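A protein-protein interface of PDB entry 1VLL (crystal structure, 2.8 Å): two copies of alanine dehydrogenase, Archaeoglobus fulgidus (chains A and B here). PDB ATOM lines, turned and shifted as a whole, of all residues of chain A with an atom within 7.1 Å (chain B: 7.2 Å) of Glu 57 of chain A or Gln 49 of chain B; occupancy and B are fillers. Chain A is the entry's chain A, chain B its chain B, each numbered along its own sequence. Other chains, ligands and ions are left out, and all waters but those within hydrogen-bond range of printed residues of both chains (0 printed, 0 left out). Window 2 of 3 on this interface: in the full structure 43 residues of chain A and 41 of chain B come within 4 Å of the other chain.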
ATOM      1  N   TYR A  55     -21.518   9.969 -18.492  1.00  0.00           N
ATOM      2  CA  TYR A  55     -21.163   8.774 -17.742  1.00  0.00           C
ATOM      3  C   TYR A  55     -21.238   8.982 -16.247  1.00  0.00           C
ATOM      4  O   TYR A  55     -20.919  10.050 -15.706  1.00  0.00           O
ATOM      5  CB  TYR A  55     -19.746   8.333 -18.084  1.00  0.00           C
ATOM      6  CG  TYR A  55     -19.580   7.721 -19.458  1.00  0.00           C
ATOM      7  CD1 TYR A  55     -19.265   8.525 -20.573  1.00  0.00           C
ATOM      8  CD2 TYR A  55     -19.713   6.335 -19.655  1.00  0.00           C
ATOM      9  CE1 TYR A  55     -19.107   7.965 -21.855  1.00  0.00           C
ATOM     10  CE2 TYR A  55     -19.552   5.760 -20.930  1.00  0.00           C
ATOM     11  CZ  TYR A  55     -19.255   6.586 -22.016  1.00  0.00           C
ATOM     12  OH  TYR A  55     -19.102   6.039 -23.263  1.00  0.00           O
ATOM     13  N   LEU A  56     -21.632   7.920 -15.574  1.00  0.00           N
ATOM     14  CA  LEU A  56     -21.627   7.883 -14.143  1.00  0.00           C
ATOM     15  C   LEU A  56     -20.876   6.593 -13.839  1.00  0.00           C
ATOM     16  O   LEU A  56     -21.332   5.511 -14.214  1.00  0.00           O
ATOM     17  CB  LEU A  56     -23.079   7.833 -13.670  1.00  0.00           C
ATOM     18  CG  LEU A  56     -23.566   8.672 -12.495  1.00  0.00           C
ATOM     19  CD1 LEU A  56     -23.073  10.109 -12.563  1.00  0.00           C
ATOM     20  CD2 LEU A  56     -25.082   8.614 -12.465  1.00  0.00           C
ATOM     21  N   GLU A  57     -19.708   6.706 -13.210  1.00  0.00           N
ATOM     22  CA  GLU A  57     -18.839   5.547 -12.976  1.00  0.00           C
ATOM     23  C   GLU A  57     -19.026   4.950 -11.595  1.00  0.00           C
ATOM     24  O   GLU A  57     -19.038   5.680 -10.607  1.00  0.00           O
ATOM     25  CB  GLU A  57     -17.368   5.934 -13.160  1.00  0.00           C
ATOM     26  CG  GLU A  57     -17.056   6.638 -14.492  1.00  0.00           C
ATOM     27  CD  GLU A  57     -16.987   5.692 -15.699  1.00  0.00           C
ATOM     28  OE1 GLU A  57     -17.616   4.602 -15.688  1.00  0.00           O
ATOM     29  OE2 GLU A  57     -16.302   6.058 -16.679  1.00  0.00           O
ATOM     30  N   PHE A  58     -19.159   3.624 -11.521  1.00  0.00           N
ATOM     31  CA  PHE A  58     -19.219   2.925 -10.230  1.00  0.00           C
ATOM     32  C   PHE A  58     -18.130   1.863 -10.125  1.00  0.00           C
ATOM     33  O   PHE A  58     -17.580   1.462 -11.150  1.00  0.00           O
ATOM     34  CB  PHE A  58     -20.594   2.295 -10.017  1.00  0.00           C
ATOM     35  CG  PHE A  58     -21.705   3.129 -10.523  1.00  0.00           C
ATOM     36  CD1 PHE A  58     -22.024   4.326  -9.900  1.00  0.00           C
ATOM     37  CD2 PHE A  58     -22.413   2.740 -11.649  1.00  0.00           C
ATOM     38  CE1 PHE A  58     -23.022   5.115 -10.393  1.00  0.00           C
ATOM     39  CE2 PHE A  58     -23.424   3.523 -12.144  1.00  0.00           C
ATOM     40  CZ  PHE A  58     -23.731   4.706 -11.515  1.00  0.00           C
ATOM     41  N   GLU A  59     -17.817   1.423  -8.897  1.00  0.00           N
ATOM     42  CA  GLU A  59     -16.874   0.324  -8.684  1.00  0.00           C
ATOM     43  C   GLU A  59     -17.290  -0.863  -9.554  1.00  0.00           C
ATOM     44  O   GLU A  59     -16.476  -1.379 -10.313  1.00  0.00           O
ATOM     45  CB  GLU A  59     -16.751  -0.080  -7.200  1.00  0.00           C
ATOM     46  N   LYS A  60     -18.561  -1.258  -9.509  1.00  0.00           N
ATOM     47  CA  LYS A  60     -18.942  -2.524 -10.130  1.00  0.00           C
ATOM     48  C   LYS A  60     -19.632  -2.401 -11.497  1.00  0.00           C
ATOM     49  O   LYS A  60     -20.178  -3.386 -11.991  1.00  0.00           O
ATOM     50  CB  LYS A  60     -19.728  -3.412  -9.137  1.00  0.00           C
ATOM     51  N   GLY A  61     -19.580  -1.214 -12.117  1.00  0.00           N
ATOM     52  CA  GLY A  61     -20.226  -0.934 -13.438  1.00  0.00           C
ATOM     53  C   GLY A  61     -20.358   0.547 -13.782  1.00  0.00           C
ATOM     54  O   GLY A  61     -19.593   1.367 -13.302  1.00  0.00           O
ATOM     55  N   ASP A  62     -21.327   0.896 -14.626  1.00  0.00           N
ATOM     56  CA  ASP A  62     -21.605   2.317 -14.975  1.00  0.00           C
ATOM     57  C   ASP A  62     -23.007   2.588 -15.536  1.00  0.00           C
ATOM     58  O   ASP A  62     -23.724   1.658 -15.897  1.00  0.00           O
ATOM     59  CB  ASP A  62     -20.544   2.885 -15.938  1.00  0.00           C
ATOM     60  CG  ASP A  62     -20.582   2.238 -17.328  1.00  0.00           C
ATOM     61  OD1 ASP A  62     -21.642   2.203 -18.012  1.00  0.00           O
ATOM     62  OD2 ASP A  62     -19.506   1.779 -17.749  1.00  0.00           O
ATOM     63  N   LEU A  63     -23.373   3.869 -15.618  1.00  0.00           N
ATOM     64  CA  LEU A  63     -24.610   4.306 -16.284  1.00  0.00           C
ATOM     65  C   LEU A  63     -24.290   5.402 -17.303  1.00  0.00           C
ATOM     66  O   LEU A  63     -23.403   6.221 -17.076  1.00  0.00           O
ATOM     67  CB  LEU A  63     -25.626   4.803 -15.252  1.00  0.00           C
ATOM     68  CG  LEU A  63     -26.474   3.747 -14.531  1.00  0.00           C
ATOM     69  CD1 LEU A  63     -26.895   4.262 -13.176  1.00  0.00           C
ATOM     70  CD2 LEU A  63     -27.689   3.342 -15.345  1.00  0.00           C
ATOM     71  N   ARG A  64     -24.987   5.413 -18.429  1.00  0.00           N
ATOM     72  CA  ARG A  64     -24.717   6.409 -19.465  1.00  0.00           C
ATOM     73  C   ARG A  64     -25.998   7.117 -19.864  1.00  0.00           C
ATOM     74  O   ARG A  64     -27.026   6.458 -20.077  1.00  0.00           O
ATOM     75  CB  ARG A  64     -24.102   5.742 -20.709  1.00  0.00           C
ATOM     76  CG  ARG A  64     -22.724   5.094 -20.496  1.00  0.00           C
ATOM     77  CD  ARG A  64     -22.438   3.941 -21.476  1.00  0.00           C
ATOM     78  N   LEU B  42     -21.373  16.080   1.523  1.00  0.00           N
ATOM     79  CA  LEU B  42     -20.712  14.951   0.893  1.00  0.00           C
ATOM     80  C   LEU B  42     -20.010  15.379  -0.368  1.00  0.00           C
ATOM     81  O   LEU B  42     -18.900  14.930  -0.646  1.00  0.00           O
ATOM     82  CB  LEU B  42     -21.691  13.821   0.602  1.00  0.00           C
ATOM     83  CG  LEU B  42     -22.190  13.062   1.847  1.00  0.00           C
ATOM     84  CD1 LEU B  42     -23.491  12.300   1.560  1.00  0.00           C
ATOM     85  CD2 LEU B  42     -21.128  12.140   2.464  1.00  0.00           C
ATOM     86  N   TYR B  43     -20.630  16.277  -1.124  1.00  0.00           N
ATOM     87  CA  TYR B  43     -20.032  16.704  -2.384  1.00  0.00           C
ATOM     88  C   TYR B  43     -18.779  17.517  -2.127  1.00  0.00           C
ATOM     89  O   TYR B  43     -17.780  17.328  -2.810  1.00  0.00           O
ATOM     90  CB  TYR B  43     -21.023  17.506  -3.218  1.00  0.00           C
ATOM     91  CG  TYR B  43     -20.537  17.856  -4.609  1.00  0.00           C
ATOM     92  CD1 TYR B  43     -20.106  16.855  -5.506  1.00  0.00           C
ATOM     93  CD2 TYR B  43     -20.524  19.185  -5.042  1.00  0.00           C
ATOM     94  CE1 TYR B  43     -19.664  17.184  -6.790  1.00  0.00           C
ATOM     95  CE2 TYR B  43     -20.093  19.522  -6.316  1.00  0.00           C
ATOM     96  CZ  TYR B  43     -19.666  18.519  -7.186  1.00  0.00           C
ATOM     97  OH  TYR B  43     -19.239  18.867  -8.449  1.00  0.00           O
ATOM     98  N   GLY B  46     -15.779  15.388  -1.511  1.00  0.00           N
ATOM     99  CA  GLY B  46     -15.391  14.471  -2.576  1.00  0.00           C
ATOM    100  C   GLY B  46     -16.064  13.105  -2.546  1.00  0.00           C
ATOM    101  O   GLY B  46     -15.579  12.162  -3.160  1.00  0.00           O
ATOM    102  N   LYS B  47     -17.189  12.998  -1.849  1.00  0.00           N
ATOM    103  CA  LYS B  47     -17.870  11.730  -1.703  1.00  0.00           C
ATOM    104  C   LYS B  47     -19.188  11.699  -2.482  1.00  0.00           C
ATOM    105  O   LYS B  47     -20.127  10.991  -2.106  1.00  0.00           O
ATOM    106  CB  LYS B  47     -18.102  11.454  -0.225  1.00  0.00           C
ATOM    107  CG  LYS B  47     -16.844  11.574   0.623  1.00  0.00           C
ATOM    108  CD  LYS B  47     -16.145  10.228   0.836  1.00  0.00           C
ATOM    109  CE  LYS B  47     -14.627  10.409   0.946  1.00  0.00           C
ATOM    110  NZ  LYS B  47     -14.028   9.663   2.100  1.00  0.00           N
ATOM    111  N   ALA B  48     -19.263  12.468  -3.562  1.00  0.00           N
ATOM    112  CA  ALA B  48     -20.434  12.453  -4.443  1.00  0.00           C
ATOM    113  C   ALA B  48     -20.042  12.795  -5.876  1.00  0.00           C
ATOM    114  O   ALA B  48     -19.153  13.598  -6.112  1.00  0.00           O
ATOM    115  CB  ALA B  48     -21.498  13.407  -3.941  1.00  0.00           C
ATOM    116  N   GLN B  49     -20.720  12.177  -6.828  1.00  0.00           N
ATOM    117  CA  GLN B  49     -20.403  12.305  -8.234  1.00  0.00           C
ATOM    118  C   GLN B  49     -21.485  13.123  -8.945  1.00  0.00           C
ATOM    119  O   GLN B  49     -22.681  12.793  -8.896  1.00  0.00           O
ATOM    120  CB  GLN B  49     -20.342  10.907  -8.805  1.00  0.00           C
ATOM    121  CG  GLN B  49     -19.147  10.607  -9.659  1.00  0.00           C
ATOM    122  CD  GLN B  49     -19.224   9.198 -10.221  1.00  0.00           C
ATOM    123  OE1 GLN B  49     -18.982   8.969 -11.415  1.00  0.00           O
ATOM    124  NE2 GLN B  49     -19.595   8.244  -9.365  1.00  0.00           N
ATOM    125  N   MET B  50     -21.073  14.211  -9.582  1.00  0.00           N
ATOM    126  CA  MET B  50     -22.003  15.044 -10.343  1.00  0.00           C
ATOM    127  C   MET B  50     -21.347  15.565 -11.620  1.00  0.00           C
ATOM    128  O   MET B  50     -20.699  16.612 -11.597  1.00  0.00           O
ATOM    129  CB  MET B  50     -22.498  16.211  -9.493  1.00  0.00           C
ATOM    130  CG  MET B  50     -23.585  17.030 -10.170  1.00  0.00           C
ATOM    131  SD  MET B  50     -24.354  18.229  -9.081  1.00  0.00           S
ATOM    132  CE  MET B  50     -23.001  19.388  -8.851  1.00  0.00           C
ATOM    133  N   PRO B  51     -21.502  14.840 -12.746  1.00  0.00           N
ATOM    134  CA  PRO B  51     -20.899  15.348 -13.972  1.00  0.00           C
ATOM    135  C   PRO B  51     -21.752  16.513 -14.485  1.00  0.00           C
ATOM    136  O   PRO B  51     -22.885  16.713 -13.994  1.00  0.00           O
ATOM    137  CB  PRO B  51     -20.967  14.147 -14.915  1.00  0.00           C
ATOM    138  CG  PRO B  51     -22.178  13.432 -14.505  1.00  0.00           C
ATOM    139  CD  PRO B  51     -22.239  13.586 -12.990  1.00  0.00           C
ATOM    140  N   PRO B  67     -27.370  13.934 -14.206  1.00  0.00           N
ATOM    141  CA  PRO B  67     -27.129  12.749 -13.393  1.00  0.00           C
ATOM    142  C   PRO B  67     -26.299  13.079 -12.163  1.00  0.00           C
ATOM    143  O   PRO B  67     -25.587  14.074 -12.157  1.00  0.00           O
ATOM    144  CB  PRO B  67     -26.337  11.843 -14.343  1.00  0.00           C
ATOM    145  CG  PRO B  67     -25.608  12.759 -15.194  1.00  0.00           C
ATOM    146  CD  PRO B  67     -26.386  14.064 -15.286  1.00  0.00           C
ATOM    147  N   ALA B  68     -26.377  12.237 -11.146  1.00  0.00           N
ATOM    148  CA  ALA B  68     -25.516  12.342  -9.970  1.00  0.00           C
ATOM    149  C   ALA B  68     -25.427  10.993  -9.303  1.00  0.00           C
ATOM    150  O   ALA B  68     -26.294  10.134  -9.507  1.00  0.00           O
ATOM    151  CB  ALA B  68     -26.084  13.335  -8.991  1.00  0.00           C
ATOM    152  N   HIS B  69     -24.398  10.825  -8.477  1.00  0.00           N
ATOM    153  CA  HIS B  69     -24.211   9.594  -7.692  1.00  0.00           C
ATOM    154  C   HIS B  69     -23.698   9.917  -6.300  1.00  0.00           C
ATOM    155  O   HIS B  69     -22.606  10.453  -6.159  1.00  0.00           O
ATOM    156  CB  HIS B  69     -23.246   8.626  -8.411  1.00  0.00           C
ATOM    157  CG  HIS B  69     -22.849   7.432  -7.593  1.00  0.00           C
ATOM    158  ND1 HIS B  69     -21.538   7.035  -7.447  1.00  0.00           N
ATOM    159  CD2 HIS B  69     -23.590   6.550  -6.875  1.00  0.00           C
ATOM    160  CE1 HIS B  69     -21.488   5.965  -6.675  1.00  0.00           C
ATOM    161  NE2 HIS B  69     -22.721   5.646  -6.318  1.00  0.00           N
ATOM    162  N   LEU B  70     -24.495   9.593  -5.284  1.00  0.00           N
ATOM    163  CA  LEU B  70     -24.092   9.725  -3.876  1.00  0.00           C
ATOM    164  C   LEU B  70     -25.022   8.930  -2.982  1.00  0.00           C
ATOM    165  O   LEU B  70     -26.073   8.455  -3.443  1.00  0.00           O
ATOM    166  CB  LEU B  70     -24.068  11.186  -3.432  1.00  0.00           C
ATOM    167  CG  LEU B  70     -25.392  11.876  -3.108  1.00  0.00           C
ATOM    168  CD1 LEU B  70     -25.133  13.106  -2.244  1.00  0.00           C
ATOM    169  CD2 LEU B  70     -26.181  12.229  -4.384  1.00  0.00           C
ATOM    170  N   TYR B  73     -26.774   5.713  -4.090  1.00  0.00           N
ATOM    171  CA  TYR B  73     -27.771   5.752  -5.143  1.00  0.00           C
ATOM    172  C   TYR B  73     -27.256   6.551  -6.320  1.00  0.00           C
ATOM    173  O   TYR B  73     -26.494   7.503  -6.147  1.00  0.00           O
ATOM    174  CB  TYR B  73     -29.061   6.389  -4.635  1.00  0.00           C
ATOM    175  CG  TYR B  73     -29.915   5.492  -3.785  1.00  0.00           C
ATOM    176  CD1 TYR B  73     -30.897   4.683  -4.365  1.00  0.00           C
ATOM    177  CD2 TYR B  73     -29.761   5.464  -2.400  1.00  0.00           C
ATOM    178  CE1 TYR B  73     -31.696   3.850  -3.596  1.00  0.00           C
ATOM    179  CE2 TYR B  73     -30.557   4.641  -1.610  1.00  0.00           C
ATOM    180  CZ  TYR B  73     -31.525   3.833  -2.216  1.00  0.00           C
ATOM    181  OH  TYR B  73     -32.324   3.022  -1.434  1.00  0.00           O
ATOM    182  N   GLY B  75     -28.806   8.407 -10.037  1.00  0.00           N
ATOM    183  CA  GLY B  75     -30.017   8.820 -10.697  1.00  0.00           C
ATOM    184  C   GLY B  75     -29.774   9.876 -11.746  1.00  0.00           C
ATOM    185  O   GLY B  75     -28.711  10.508 -11.794  1.00  0.00           O
ATOM    186  N   PRO B 102     -26.345   1.653  -7.854  1.00  0.00           N
ATOM    187  CA  PRO B 102     -24.980   1.660  -8.388  1.00  0.00           C
ATOM    188  C   PRO B 102     -24.376   0.267  -8.489  1.00  0.00           C
ATOM    189  O   PRO B 102     -23.336   0.107  -9.123  1.00  0.00           O
ATOM    190  CB  PRO B 102     -24.190   2.489  -7.366  1.00  0.00           C
ATOM    191  CG  PRO B 102     -25.211   3.225  -6.578  1.00  0.00           C
ATOM    192  CD  PRO B 102     -26.418   2.328  -6.550  1.00  0.00           C
ATOM    193  N   ALA B 306     -27.625  18.485  -9.199  1.00  0.00           N
ATOM    194  CA  ALA B 306     -28.304  17.192  -9.380  1.00  0.00           C
ATOM    195  C   ALA B 306     -28.253  16.302  -8.139  1.00  0.00           C
ATOM    196  O   ALA B 306     -29.145  15.497  -7.908  1.00  0.00           O
ATOM    197  CB  ALA B 306     -27.747  16.471 -10.587  1.00  0.00           C
ATOM    198  N   ILE B 307     -27.206  16.464  -7.345  1.00  0.00           N
ATOM    199  CA  ILE B 307     -27.066  15.723  -6.105  1.00  0.00           C
ATOM    200  C   ILE B 307     -28.234  16.016  -5.152  1.00  0.00           C
ATOM    201  O   ILE B 307     -28.746  15.114  -4.502  1.00  0.00           O
ATOM    202  CB  ILE B 307     -25.684  15.962  -5.453  1.00  0.00           C
ATOM    203  CG1 ILE B 307     -25.452  17.445  -5.148  1.00  0.00           C
ATOM    204  CG2 ILE B 307     -24.587  15.497  -6.385  1.00  0.00           C
ATOM    205  CD1 ILE B 307     -24.301  17.684  -4.196  1.00  0.00           C
ATOM    206  N   VAL B 310     -31.008  13.643  -6.504  1.00  0.00           N
ATOM    207  CA  VAL B 310     -30.881  12.226  -6.186  1.00  0.00           C
ATOM    208  C   VAL B 310     -31.104  12.005  -4.689  1.00  0.00           C
ATOM    209  O   VAL B 310     -31.919  11.168  -4.290  1.00  0.00           O
ATOM    210  CB  VAL B 310     -29.545  11.644  -6.631  1.00  0.00           C
ATOM    211  CG1 VAL B 310     -29.357  10.221  -6.067  1.00  0.00           C
ATOM    212  CG2 VAL B 310     -29.450  11.652  -8.167  1.00  0.00           C
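The backbone carbonyl oxygen (O) of Glu 57 of chain A sits at hydrogen-bond distance from the side-chain amide nitrogen (NE2) of Gln 49 of chain B (2.9 Å).
N of Leu 56 of chain A lies within hydrogen-bond range of O of Leu 63 of chain A. The backbone NH (N) of Gln 49 of chain B lies within hydrogen-bond range of the backbone carbonyl oxygen (O) of His 69 of chain B, at 2.6 Å. The backbone carbonyl oxygen (O) of Gly 75 of chain B sits at hydrogen-bond distance from the backbone NH (N) of Ala 68 of chain B (3.0 Å).
Among the printed residues, merely in contact across the chains: Leu 56 of chain A with Ala 68 of chain B (3.5 Å), Leu 56 of chain A with Pro 51 of chain B (3.6 Å), Phe 58 of chain A with Pro 102 of chain B (3.6 Å), Phe 58 of chain A with His 69 of chain B (3.6 Å), Tyr 55 of chain A with Pro 51 of chain B (3.8 Å), Leu 56 of chain A with Gln 49 of chain B (3.9 Å) and Leu 56 of chain A with Pro 67 of chain B (3.9 Å).
Glu 57 of chain A touches one residue of chain B. Printed residues of chain B within 4 Å of Phe 58 of chain A: His 69 and Pro 102. Of chain A, only Leu 56 (3.9 Å) and Glu 57 (2.9 Å) come within 4 Å of Gln 49 of chain B. Printed residues of chain A within 4 Å of Pro 51 of chain B: Tyr 55 and Leu 56. Of the printed residues of chain A, Pro 67 of chain B touches Leu 56. Printed residues of chain A within 4 Å of Ala 68 of chain B: Leu 56 (3.5 Å). Printed residues of chain A within 4 Å of Pro 102 of chain B: Phe 58 (3.6 Å). The nearest residue of chain A that does not touch Gln 49 of chain B is Phe 58 of chain A (4.6 Å).
Printed residues of chain B that touch a printed residue of chain A: Gln 49, Pro 51, Pro 67, Ala 68, His 69 and Pro 102. Hydrophobic or aromatic side chains of chain B that line the printed part of chain A: Pro 51, Pro 67, His 69 and Pro 102. Along chain B the printed residues that touch a printed residue of chain A span positions 49 to 102. Among the printed residues, no Asp or Glu carboxylate lies within 4 Å of a Lys or Arg side-chain nitrogen of the other chain.
No position is printed for both chains. Of the 8 pairs that touch across the chains among the printed residues, none has its exchanged pair printed and touching as well.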
